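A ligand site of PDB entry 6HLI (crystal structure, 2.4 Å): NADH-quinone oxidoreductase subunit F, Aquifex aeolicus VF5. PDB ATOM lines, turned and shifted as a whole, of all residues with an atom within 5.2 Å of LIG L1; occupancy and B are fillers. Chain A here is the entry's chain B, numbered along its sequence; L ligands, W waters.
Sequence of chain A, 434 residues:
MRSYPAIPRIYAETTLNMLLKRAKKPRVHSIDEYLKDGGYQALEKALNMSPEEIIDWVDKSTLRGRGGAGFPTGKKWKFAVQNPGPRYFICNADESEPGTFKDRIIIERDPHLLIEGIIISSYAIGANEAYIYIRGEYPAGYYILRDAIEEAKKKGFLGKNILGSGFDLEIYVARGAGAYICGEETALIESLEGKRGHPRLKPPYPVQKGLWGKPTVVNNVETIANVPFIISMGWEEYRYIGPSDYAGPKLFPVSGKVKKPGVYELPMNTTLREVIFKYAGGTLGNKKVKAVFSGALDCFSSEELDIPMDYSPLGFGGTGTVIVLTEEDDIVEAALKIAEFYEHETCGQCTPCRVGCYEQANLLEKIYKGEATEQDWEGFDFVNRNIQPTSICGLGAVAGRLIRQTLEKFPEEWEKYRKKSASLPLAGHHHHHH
OE1 of Glu 185 sits at hydrogen-bond distance from O5 of LIG L1, 2.7 Å away.
An oxygen (O5) of LIG L1 sits at hydrogen-bond distance from the side-chain amino group (NZ) of Lys 76, 2.7 Å away.
The backbone carbonyl oxygen of Gly 68 lies within hydrogen-bond range of an oxygen (O12) of LIG L1 (2.9 Å).
An oxygen (O3) of LG2 L2 is in hydrogen-bond range of the backbone NH of Glu 185 (3.1 Å).
An oxygen (O8) of LG2 L2 is in salt-bridge range of the side-chain amino group (NZ) of Lys 76, 2.7 Å away.
The backbone NH of Gly 67 sits at hydrogen-bond distance from an oxygen (O7) of LG2 L2, 2.8 Å away.
N of Glu 95 sits at hydrogen-bond distance from O2 of LG2 L2, 2.9 Å away.
An oxygen (O9) of LG2 L2 is in hydrogen-bond range of the backbone NH (N) of Asn 220 (3.0 Å).
ND2 of Asn 220 sits at hydrogen-bond distance from O1 of LG2 L2 (2.8 Å).
The backbone NH (N) of Arg 66 lies within hydrogen-bond range of an oxygen (O7) of LG2 L2, at 3.2 Å.
O3 of LG2 L2 lies within hydrogen-bond range of O9 of LIG L1, 2.8 Å away.
The backbone carbonyl oxygen (O) of Val 218 is in hydrogen-bond range of the side-chain amino group (NZ) of Lys 76 (2.7 Å).
The side-chain hydroxyl of Tyr 180 is in hydrogen-bond range of the side-chain carboxylate of Glu 97 (2.9 Å).
OG1 of Thr 100 lies close to O of Glu 97 (3.3 Å).
OE2 of Glu 95 sits at hydrogen-bond distance from N of Asp 103 (2.8 Å).
The side-chain carboxylate (OE2) of Glu 95 lies within hydrogen-bond range of the backbone NH (N) of Lys 102, at 3.0 Å.
O of Gly 67 sits close to O11 of LIG L1 (3.2 Å).
CB of Ala 69 touches O7 of LIG L1, at 3.2 Å.
Phe 71 touches LIG L1 (CG to O4, 3.3 Å).
Phe 79 touches LIG L1 (CD2 to C9, 3.8 Å).
Glu 95 touches LIG L1 (CA to O14, 3.2 Å).
Ser 96 touches LIG L1.
CB of Glu 97 touches C19 of LIG L1, at 3.2 Å.
CG2 of Thr 100 touches O14 of LIG L1, 3.9 Å away.
Tyr 180 touches LIG L1 (OH to C20, 3.0 Å).
Tyr 205 touches LIG L1.
Pro 206 touches LIG L1 (CD to O6, 3.7 Å).
CG2 of Val 207 touches C9 of LIG L1, 3.6 Å away.
Thr 319 touches LIG L1 (CG2 to N7, 3.4 Å).
16 residues have an atom within 4 Å of LIG L1: Gly 67, Gly 68, Ala 69, Phe 71, Lys 76, Phe 79, Glu 95, Ser 96, Glu 97, Thr 100, Tyr 180, Glu 185, Tyr 205, Pro 206, Val 207 and Thr 319.
The nearest printed residue that does not touch LIG L1 is Leu 297 (4.003 Å).
Water W1 lies within hydrogen-bond range of O8 of LIG L1, N of Gly 394 and OE2 of Glu 184.
Water W2 lies within hydrogen-bond range of the side-chain carboxylate (OE2) of Glu 95 (2.6 Å), the side-chain carboxylate (OD2) of Asp 103 (2.7 Å), a nitrogen (N7) of LIG L1 (2.8 Å) and the side-chain amino group (NZ) of Lys 102 (3.3 Å).
Water W3 lies within hydrogen-bond range of O9 of LIG L1, OE2 of Glu 185 and OE2 of Glu 184.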
ATOM      1  N   ARG A  66       5.908  21.177   3.532  1.00  0.00           N
ATOM      2  CA  ARG A  66       6.477  20.872   4.855  1.00  0.00           C
ATOM      3  C   ARG A  66       5.545  21.272   6.017  1.00  0.00           C
ATOM      4  O   ARG A  66       5.897  21.144   7.190  1.00  0.00           O
ATOM      5  CB  ARG A  66       7.874  21.515   5.012  1.00  0.00           C
ATOM      6  CG  ARG A  66       8.938  21.001   4.034  1.00  0.00           C
ATOM      7  CD  ARG A  66       9.239  19.522   4.175  1.00  0.00           C
ATOM      8  NE  ARG A  66      10.469  19.170   3.461  1.00  0.00           N
ATOM      9  CZ  ARG A  66      10.529  18.400   2.382  1.00  0.00           C
ATOM     10  NH1 ARG A  66      11.702  18.145   1.808  1.00  0.00           N
ATOM     11  NH2 ARG A  66       9.420  17.850   1.875  1.00  0.00           N
ATOM     12  N   GLY A  67       4.367  21.758   5.675  1.00  0.00           N
ATOM     13  CA  GLY A  67       3.388  22.194   6.673  1.00  0.00           C
ATOM     14  C   GLY A  67       2.416  21.107   7.071  1.00  0.00           C
ATOM     15  O   GLY A  67       1.288  21.430   7.452  1.00  0.00           O
ATOM     16  N   GLY A  68       2.799  19.834   6.932  1.00  0.00           N
ATOM     17  CA  GLY A  68       2.007  18.687   7.374  1.00  0.00           C
ATOM     18  C   GLY A  68       1.235  17.831   6.398  1.00  0.00           C
ATOM     19  O   GLY A  68       1.098  16.628   6.631  1.00  0.00           O
ATOM     20  N   ALA A  69       0.645  18.423   5.360  1.00  0.00           N
ATOM     21  CA  ALA A  69      -0.158  17.680   4.401  1.00  0.00           C
ATOM     22  C   ALA A  69       0.647  17.058   3.238  1.00  0.00           C
ATOM     23  O   ALA A  69       0.142  16.172   2.547  1.00  0.00           O
ATOM     24  CB  ALA A  69      -1.285  18.548   3.894  1.00  0.00           C
ATOM     25  N   PHE A  71       1.663  18.170   0.167  1.00  0.00           N
ATOM     26  CA  PHE A  71       1.203  18.324  -1.223  1.00  0.00           C
ATOM     27  C   PHE A  71       2.387  18.716  -2.151  1.00  0.00           C
ATOM     28  O   PHE A  71       3.207  19.535  -1.730  1.00  0.00           O
ATOM     29  CB  PHE A  71       0.095  19.375  -1.305  1.00  0.00           C
ATOM     30  CG  PHE A  71      -0.660  19.409  -2.609  1.00  0.00           C
ATOM     31  CD1 PHE A  71      -1.703  18.530  -2.842  1.00  0.00           C
ATOM     32  CD2 PHE A  71      -0.325  20.326  -3.587  1.00  0.00           C
ATOM     33  CE1 PHE A  71      -2.389  18.557  -4.056  1.00  0.00           C
ATOM     34  CE2 PHE A  71      -1.023  20.350  -4.812  1.00  0.00           C
ATOM     35  CZ  PHE A  71      -2.051  19.461  -5.032  1.00  0.00           C
ATOM     36  N   LYS A  76       1.175  22.492  -6.951  1.00  0.00           N
ATOM     37  CA  LYS A  76       0.424  23.614  -6.380  1.00  0.00           C
ATOM     38  C   LYS A  76       0.633  24.919  -7.173  1.00  0.00           C
ATOM     39  O   LYS A  76      -0.333  25.621  -7.441  1.00  0.00           O
ATOM     40  CB  LYS A  76       0.771  23.822  -4.904  1.00  0.00           C
ATOM     41  CG  LYS A  76      -0.304  24.628  -4.153  1.00  0.00           C
ATOM     42  CD  LYS A  76       0.167  25.159  -2.780  1.00  0.00           C
ATOM     43  CE  LYS A  76       0.385  24.025  -1.793  1.00  0.00           C
ATOM     44  NZ  LYS A  76       0.441  24.521  -0.414  1.00  0.00           N
ATOM     45  N   PHE A  79      -1.178  24.765 -10.600  1.00  0.00           N
ATOM     46  CA  PHE A  79      -2.609  25.025 -10.447  1.00  0.00           C
ATOM     47  C   PHE A  79      -2.910  26.527 -10.417  1.00  0.00           C
ATOM     48  O   PHE A  79      -3.788  26.973 -11.133  1.00  0.00           O
ATOM     49  CB  PHE A  79      -3.198  24.335  -9.198  1.00  0.00           C
ATOM     50  CG  PHE A  79      -3.587  22.881  -9.310  1.00  0.00           C
ATOM     51  CD1 PHE A  79      -4.556  22.464 -10.220  1.00  0.00           C
ATOM     52  CD2 PHE A  79      -3.083  21.938  -8.418  1.00  0.00           C
ATOM     53  CE1 PHE A  79      -4.926  21.123 -10.316  1.00  0.00           C
ATOM     54  CE2 PHE A  79      -3.471  20.580  -8.509  1.00  0.00           C
ATOM     55  CZ  PHE A  79      -4.388  20.189  -9.454  1.00  0.00           C
ATOM     56  N   GLU A  95       3.046  28.231  12.662  1.00  0.00           N
ATOM     57  CA  GLU A  95       3.584  27.161  13.538  1.00  0.00           C
ATOM     58  C   GLU A  95       3.076  27.165  15.024  1.00  0.00           C
ATOM     59  O   GLU A  95       3.737  27.704  15.910  1.00  0.00           O
ATOM     60  CB  GLU A  95       5.134  27.164  13.481  1.00  0.00           C
ATOM     61  CG  GLU A  95       5.764  25.936  14.098  1.00  0.00           C
ATOM     62  CD  GLU A  95       7.263  25.890  13.956  1.00  0.00           C
ATOM     63  OE1 GLU A  95       7.945  26.761  14.545  1.00  0.00           O
ATOM     64  OE2 GLU A  95       7.768  24.983  13.271  1.00  0.00           O
ATOM     65  N   SER A  96       1.898  26.600  15.244  1.00  0.00           N
ATOM     66  CA  SER A  96       1.229  26.540  16.550  1.00  0.00           C
ATOM     67  C   SER A  96       0.965  25.073  17.008  1.00  0.00           C
ATOM     68  O   SER A  96       0.417  24.852  18.093  1.00  0.00           O
ATOM     69  CB  SER A  96      -0.062  27.370  16.536  1.00  0.00           C
ATOM     70  OG  SER A  96       0.082  28.730  16.124  1.00  0.00           O
ATOM     71  N   GLU A  97       1.399  24.091  16.173  1.00  0.00           N
ATOM     72  CA  GLU A  97       1.271  22.651  16.405  1.00  0.00           C
ATOM     73  C   GLU A  97       2.074  22.187  17.617  1.00  0.00           C
ATOM     74  O   GLU A  97       3.293  22.377  17.618  1.00  0.00           O
ATOM     75  CB  GLU A  97       1.722  21.895  15.131  1.00  0.00           C
ATOM     76  CG  GLU A  97       1.554  20.363  15.153  1.00  0.00           C
ATOM     77  CD  GLU A  97       0.169  19.747  15.127  1.00  0.00           C
ATOM     78  OE1 GLU A  97       0.092  18.500  15.066  1.00  0.00           O
ATOM     79  OE2 GLU A  97      -0.835  20.498  15.163  1.00  0.00           O
ATOM     80  N   THR A 100       6.048  21.317  17.554  1.00  0.00           N
ATOM     81  CA  THR A 100       6.575  21.830  16.295  1.00  0.00           C
ATOM     82  C   THR A 100       7.208  23.203  16.492  1.00  0.00           C
ATOM     83  O   THR A 100       6.517  24.177  16.807  1.00  0.00           O
ATOM     84  CB  THR A 100       5.489  21.773  15.239  1.00  0.00           C
ATOM     85  OG1 THR A 100       4.776  20.519  15.386  1.00  0.00           O
ATOM     86  CG2 THR A 100       6.032  21.969  13.802  1.00  0.00           C
ATOM     87  N   LYS A 102      10.316  23.887  14.370  1.00  0.00           N
ATOM     88  CA  LYS A 102      11.289  23.804  13.265  1.00  0.00           C
ATOM     89  C   LYS A 102      11.377  25.090  12.417  1.00  0.00           C
ATOM     90  O   LYS A 102      12.484  25.494  12.046  1.00  0.00           O
ATOM     91  CB  LYS A 102      11.022  22.574  12.362  1.00  0.00           C
ATOM     92  CG  LYS A 102       9.636  22.572  11.743  1.00  0.00           C
ATOM     93  CD  LYS A 102       9.366  21.434  10.781  1.00  0.00           C
ATOM     94  CE  LYS A 102       7.971  21.573  10.206  1.00  0.00           C
ATOM     95  NZ  LYS A 102       7.867  22.593   9.101  1.00  0.00           N
ATOM     96  N   ASP A 103      10.217  25.673  12.078  1.00  0.00           N
ATOM     97  CA  ASP A 103      10.123  26.876  11.246  1.00  0.00           C
ATOM     98  C   ASP A 103      10.788  28.086  11.915  1.00  0.00           C
ATOM     99  O   ASP A 103      11.481  28.839  11.235  1.00  0.00           O
ATOM    100  CB  ASP A 103       8.668  27.219  10.918  1.00  0.00           C
ATOM    101  CG  ASP A 103       7.927  26.184  10.082  1.00  0.00           C
ATOM    102  OD1 ASP A 103       8.590  25.322   9.500  1.00  0.00           O
ATOM    103  OD2 ASP A 103       6.701  26.250  10.006  1.00  0.00           O
ATOM    104  N   TYR A 180      -4.628  29.134  16.735  1.00  0.00           N
ATOM    105  CA  TYR A 180      -4.037  27.972  16.054  1.00  0.00           C
ATOM    106  C   TYR A 180      -4.643  27.743  14.664  1.00  0.00           C
ATOM    107  O   TYR A 180      -3.917  27.426  13.714  1.00  0.00           O
ATOM    108  CB  TYR A 180      -4.219  26.708  16.908  1.00  0.00           C
ATOM    109  CG  TYR A 180      -3.959  25.411  16.183  1.00  0.00           C
ATOM    110  CD1 TYR A 180      -2.674  25.078  15.762  1.00  0.00           C
ATOM    111  CD2 TYR A 180      -4.987  24.514  15.907  1.00  0.00           C
ATOM    112  CE1 TYR A 180      -2.407  23.881  15.085  1.00  0.00           C
ATOM    113  CE2 TYR A 180      -4.742  23.304  15.265  1.00  0.00           C
ATOM    114  CZ  TYR A 180      -3.452  23.000  14.838  1.00  0.00           C
ATOM    115  OH  TYR A 180      -3.163  21.824  14.184  1.00  0.00           O
ATOM    116  N   GLU A 184      -4.358  27.228   9.337  1.00  0.00           N
ATOM    117  CA  GLU A 184      -5.121  26.633   8.260  1.00  0.00           C
ATOM    118  C   GLU A 184      -5.192  27.764   7.188  1.00  0.00           C
ATOM    119  O   GLU A 184      -5.585  28.899   7.497  1.00  0.00           O
ATOM    120  CB  GLU A 184      -6.507  26.173   8.747  1.00  0.00           C
ATOM    121  CG  GLU A 184      -7.273  25.329   7.753  1.00  0.00           C
ATOM    122  CD  GLU A 184      -7.988  26.090   6.660  1.00  0.00           C
ATOM    123  OE1 GLU A 184      -8.345  27.268   6.875  1.00  0.00           O
ATOM    124  OE2 GLU A 184      -8.189  25.494   5.570  1.00  0.00           O
ATOM    125  N   GLU A 185      -4.714  27.476   5.987  1.00  0.00           N
ATOM    126  CA  GLU A 185      -4.563  28.420   4.877  1.00  0.00           C
ATOM    127  C   GLU A 185      -5.720  29.393   4.598  1.00  0.00           C
ATOM    128  O   GLU A 185      -5.445  30.567   4.419  1.00  0.00           O
ATOM    129  CB  GLU A 185      -4.198  27.684   3.593  1.00  0.00           C
ATOM    130  CG  GLU A 185      -5.155  26.577   3.229  1.00  0.00           C
ATOM    131  CD  GLU A 185      -4.847  25.956   1.892  1.00  0.00           C
ATOM    132  OE1 GLU A 185      -3.742  26.208   1.358  1.00  0.00           O
ATOM    133  OE2 GLU A 185      -5.728  25.231   1.380  1.00  0.00           O
ATOM    134  N   TYR A 205     -10.005  26.030  -3.763  1.00  0.00           N
ATOM    135  CA  TYR A 205      -8.692  26.011  -3.113  1.00  0.00           C
ATOM    136  C   TYR A 205      -8.052  27.370  -3.300  1.00  0.00           C
ATOM    137  O   TYR A 205      -8.405  28.035  -4.290  1.00  0.00           O
ATOM    138  CB  TYR A 205      -7.813  24.859  -3.629  1.00  0.00           C
ATOM    139  CG  TYR A 205      -8.272  23.518  -3.084  1.00  0.00           C
ATOM    140  CD1 TYR A 205      -7.924  23.116  -1.794  1.00  0.00           C
ATOM    141  CD2 TYR A 205      -9.083  22.670  -3.837  1.00  0.00           C
ATOM    142  CE1 TYR A 205      -8.361  21.891  -1.272  1.00  0.00           C
ATOM    143  CE2 TYR A 205      -9.503  21.437  -3.338  1.00  0.00           C
ATOM    144  CZ  TYR A 205      -9.149  21.065  -2.054  1.00  0.00           C
ATOM    145  OH  TYR A 205      -9.593  19.857  -1.555  1.00  0.00           O
ATOM    146  N   PRO A 206      -7.178  27.847  -2.369  1.00  0.00           N
ATOM    147  CA  PRO A 206      -6.623  29.213  -2.513  1.00  0.00           C
ATOM    148  C   PRO A 206      -5.997  29.558  -3.850  1.00  0.00           C
ATOM    149  O   PRO A 206      -6.020  30.730  -4.238  1.00  0.00           O
ATOM    150  CB  PRO A 206      -5.607  29.291  -1.382  1.00  0.00           C
ATOM    151  CG  PRO A 206      -6.170  28.388  -0.352  1.00  0.00           C
ATOM    152  CD  PRO A 206      -6.688  27.222  -1.133  1.00  0.00           C
ATOM    153  N   VAL A 207      -5.443  28.546  -4.563  1.00  0.00           N
ATOM    154  CA  VAL A 207      -4.801  28.723  -5.876  1.00  0.00           C
ATOM    155  C   VAL A 207      -5.805  29.218  -6.941  1.00  0.00           C
ATOM    156  O   VAL A 207      -5.402  29.780  -7.961  1.00  0.00           O
ATOM    157  CB  VAL A 207      -4.014  27.459  -6.307  1.00  0.00           C
ATOM    158  CG1 VAL A 207      -2.791  27.219  -5.423  1.00  0.00           C
ATOM    159  CG2 VAL A 207      -4.911  26.224  -6.349  1.00  0.00           C
ATOM    160  N   VAL A 218      -0.175  29.372  -0.883  1.00  0.00           N
ATOM    161  CA  VAL A 218       0.219  29.330   0.509  1.00  0.00           C
ATOM    162  C   VAL A 218       1.213  28.195   0.690  1.00  0.00           C
ATOM    163  O   VAL A 218       0.898  27.067   0.338  1.00  0.00           O
ATOM    164  CB  VAL A 218      -0.947  29.248   1.521  1.00  0.00           C
ATOM    165  CG1 VAL A 218      -0.418  29.405   2.944  1.00  0.00           C
ATOM    166  CG2 VAL A 218      -2.020  30.318   1.212  1.00  0.00           C
ATOM    167  N   ASN A 220       4.516  26.714   3.483  1.00  0.00           N
ATOM    168  CA  ASN A 220       5.134  26.677   4.812  1.00  0.00           C
ATOM    169  C   ASN A 220       6.572  27.186   4.730  1.00  0.00           C
ATOM    170  O   ASN A 220       7.220  26.962   3.705  1.00  0.00           O
ATOM    171  CB  ASN A 220       5.116  25.205   5.321  1.00  0.00           C
ATOM    172  CG  ASN A 220       5.900  24.968   6.580  1.00  0.00           C
ATOM    173  OD1 ASN A 220       6.978  24.406   6.574  1.00  0.00           O
ATOM    174  ND2 ASN A 220       5.397  25.456   7.682  1.00  0.00           N
ATOM    175  N   LEU A 297      -1.327  14.876  16.228  1.00  0.00           N
ATOM    176  CA  LEU A 297      -1.871  14.068  15.132  1.00  0.00           C
ATOM    177  C   LEU A 297      -1.778  12.551  15.345  1.00  0.00           C
ATOM    178  O   LEU A 297      -2.831  11.899  15.411  1.00  0.00           O
ATOM    179  CB  LEU A 297      -1.179  14.499  13.827  1.00  0.00           C
ATOM    180  CG  LEU A 297      -1.802  14.094  12.490  1.00  0.00           C
ATOM    181  CD1 LEU A 297      -3.134  14.720  12.298  1.00  0.00           C
ATOM    182  CD2 LEU A 297      -0.852  14.418  11.324  1.00  0.00           C
ATOM    183  N   GLY A 318       3.383  13.756   8.622  1.00  0.00           N
ATOM    184  CA  GLY A 318       3.132  14.990   9.348  1.00  0.00           C
ATOM    185  C   GLY A 318       4.222  16.004   9.078  1.00  0.00           C
ATOM    186  O   GLY A 318       4.682  16.104   7.941  1.00  0.00           O
ATOM    187  N   THR A 319       4.653  16.722  10.115  1.00  0.00           N
ATOM    188  CA  THR A 319       5.725  17.718  10.004  1.00  0.00           C
ATOM    189  C   THR A 319       7.013  17.128  10.518  1.00  0.00           C
ATOM    190  O   THR A 319       8.014  17.833  10.634  1.00  0.00           O
ATOM    191  CB  THR A 319       5.354  19.054  10.713  1.00  0.00           C
ATOM    192  OG1 THR A 319       5.227  18.885  12.137  1.00  0.00           O
ATOM    193  CG2 THR A 319       4.129  19.719  10.147  1.00  0.00           C
ATOM    194  N   GLY A 394      -9.513  20.696   8.366  1.00  0.00           N
ATOM    195  CA  GLY A 394      -8.738  19.582   8.910  1.00  0.00           C
ATOM    196  C   GLY A 394      -8.737  19.415  10.413  1.00  0.00           C
ATOM    197  O   GLY A 394      -8.439  18.320  10.892  1.00  0.00           O
HETATM  198  P1  LIG L   1      -4.693  19.461   2.642  1.00  0.00           P
HETATM  199  O1  LIG L   1      -4.361  18.038   2.405  1.00  0.00           O
HETATM  200  O2  LIG L   1      -6.195  19.664   2.454  1.00  0.00           O
HETATM  201  O3  LIG L   1      -4.007  20.432   1.550  1.00  0.00           O
HETATM  202  C1  LIG L   1      -2.622  20.794   1.617  1.00  0.00           C
HETATM  203  C2  LIG L   1      -2.294  21.848   0.589  1.00  0.00           C
HETATM  204  O4  LIG L   1      -2.563  21.349  -0.730  1.00  0.00           O
HETATM  205  C3  LIG L   1      -3.020  23.194   0.704  1.00  0.00           C
HETATM  206  O5  LIG L   1      -2.101  24.268   0.543  1.00  0.00           O
HETATM  207  C4  LIG L   1      -4.037  23.179  -0.443  1.00  0.00           C
HETATM  208  O6  LIG L   1      -4.297  24.445  -1.037  1.00  0.00           O
HETATM  209  C5  LIG L   1      -3.378  22.251  -1.458  1.00  0.00           C
HETATM  210  N1  LIG L   1      -4.333  21.474  -2.218  1.00  0.00           N
HETATM  211  C6  LIG L   1      -4.900  20.278  -1.866  1.00  0.00           C
HETATM  212  N2  LIG L   1      -5.675  19.759  -2.794  1.00  0.00           N
HETATM  213  C7  LIG L   1      -5.608  20.685  -3.828  1.00  0.00           C
HETATM  214  C8  LIG L   1      -6.204  20.727  -5.096  1.00  0.00           C
HETATM  215  N3  LIG L   1      -6.957  19.742  -5.596  1.00  0.00           N
HETATM  216  N4  LIG L   1      -5.975  21.821  -5.872  1.00  0.00           N
HETATM  217  C9  LIG L   1      -5.183  22.795  -5.392  1.00  0.00           C
HETATM  218  N5  LIG L   1      -4.547  22.856  -4.213  1.00  0.00           N
HETATM  219  C10 LIG L   1      -4.805  21.759  -3.481  1.00  0.00           C
HETATM  220  O7  LIG L   1      -4.245  19.802   4.137  1.00  0.00           O
HETATM  221  P2  LIG L   1      -4.586  20.895   5.257  1.00  0.00           P
HETATM  222  O8  LIG L   1      -5.955  20.608   5.728  1.00  0.00           O
HETATM  223  O9  LIG L   1      -4.272  22.234   4.702  1.00  0.00           O
HETATM  224  O10 LIG L   1      -3.475  20.642   6.395  1.00  0.00           O
HETATM  225  C11 LIG L   1      -3.458  19.620   7.422  1.00  0.00           C
HETATM  226  C12 LIG L   1      -2.048  19.430   7.930  1.00  0.00           C
HETATM  227  O11 LIG L   1      -1.580  20.630   8.584  1.00  0.00           O
HETATM  228  C13 LIG L   1      -1.803  18.290   8.942  1.00  0.00           C
HETATM  229  O12 LIG L   1      -1.196  17.120   8.391  1.00  0.00           O
HETATM  230  C14 LIG L   1      -0.881  18.915  10.009  1.00  0.00           C
HETATM  231  O13 LIG L   1       0.295  18.165  10.270  1.00  0.00           O
HETATM  232  C15 LIG L   1      -0.507  20.256   9.399  1.00  0.00           C
HETATM  233  N6  LIG L   1      -0.250  21.389  10.451  1.00  0.00           N
HETATM  234  C16 LIG L   1       0.993  21.910  10.474  1.00  0.00           C
HETATM  235  C17 LIG L   1       1.361  22.767  11.492  1.00  0.00           C
HETATM  236  C18 LIG L   1       2.753  23.365  11.592  1.00  0.00           C
HETATM  237  O14 LIG L   1       3.013  24.145  12.533  1.00  0.00           O
HETATM  238  N7  LIG L   1       3.641  23.042  10.680  1.00  0.00           N
HETATM  239  C19 LIG L   1       0.429  23.072  12.481  1.00  0.00           C
HETATM  240  C20 LIG L   1      -0.836  22.522  12.430  1.00  0.00           C
HETATM  241  C21 LIG L   1      -1.170  21.690  11.395  1.00  0.00           C
HETATM  242  N1  LG2 L   2       0.693  24.922   7.860  1.00  0.00           N
HETATM  243  C1  LG2 L   2       1.771  25.650   8.279  1.00  0.00           C
HETATM  244  O1  LG2 L   2       2.676  25.961   7.501  1.00  0.00           O
HETATM  245  N2  LG2 L   2       1.807  26.161   9.572  1.00  0.00           N
HETATM  246  C2  LG2 L   2       0.806  26.060  10.522  1.00  0.00           C
HETATM  247  O2  LG2 L   2       0.984  26.490  11.650  1.00  0.00           O
HETATM  248  C3  LG2 L   2      -0.376  25.344  10.054  1.00  0.00           C
HETATM  249  N3  LG2 L   2      -1.398  25.256  10.853  1.00  0.00           N
HETATM  250  C4  LG2 L   2      -2.508  24.521  10.427  1.00  0.00           C
HETATM  251  C5  LG2 L   2      -3.592  24.390  11.302  1.00  0.00           C
HETATM  252  C6  LG2 L   2      -4.703  23.622  10.954  1.00  0.00           C
HETATM  253  C7  LG2 L   2      -5.868  23.533  11.909  1.00  0.00           C
HETATM  254  C8  LG2 L   2      -4.734  22.973   9.697  1.00  0.00           C
HETATM  255  C9  LG2 L   2      -5.928  22.151   9.256  1.00  0.00           C
HETATM  256  C10 LG2 L   2      -3.665  23.123   8.814  1.00  0.00           C
HETATM  257  C11 LG2 L   2      -2.554  23.890   9.162  1.00  0.00           C
HETATM  258  N4  LG2 L   2      -1.445  24.061   8.284  1.00  0.00           N
HETATM  259  C12 LG2 L   2      -0.336  24.780   8.698  1.00  0.00           C
HETATM  260  C13 LG2 L   2      -1.534  23.573   6.895  1.00  0.00           C
HETATM  261  C14 LG2 L   2      -2.001  24.663   5.922  1.00  0.00           C
HETATM  262  O3  LG2 L   2      -3.437  24.674   5.841  1.00  0.00           O
HETATM  263  C15 LG2 L   2      -1.395  24.505   4.524  1.00  0.00           C
HETATM  264  O4  LG2 L   2      -1.676  23.195   4.014  1.00  0.00           O
HETATM  265  C16 LG2 L   2       0.106  24.794   4.400  1.00  0.00           C
HETATM  266  O5  LG2 L   2       0.456  26.042   5.010  1.00  0.00           O
HETATM  267  C17 LG2 L   2       0.526  24.803   2.950  1.00  0.00           C
HETATM  268  O6  LG2 L   2       1.958  24.829   2.830  1.00  0.00           O
HETATM  269  P1  LG2 L   2       2.825  23.579   2.296  1.00  0.00           P
HETATM  270  O7  LG2 L   2       2.971  22.440   3.326  1.00  0.00           O
HETATM  271  O8  LG2 L   2       2.202  23.071   0.998  1.00  0.00           O
HETATM  272  O9  LG2 L   2       4.179  24.192   1.957  1.00  0.00           O
HETATM  273  O   HOH W   1      -7.820  22.480   6.404  1.00  0.00           O
HETATM  274  O   HOH W   2       6.068  24.064  11.510  1.00  0.00           O
HETATM  275  O   HOH W   3      -6.777  23.181   3.467  1.00  0.00           O
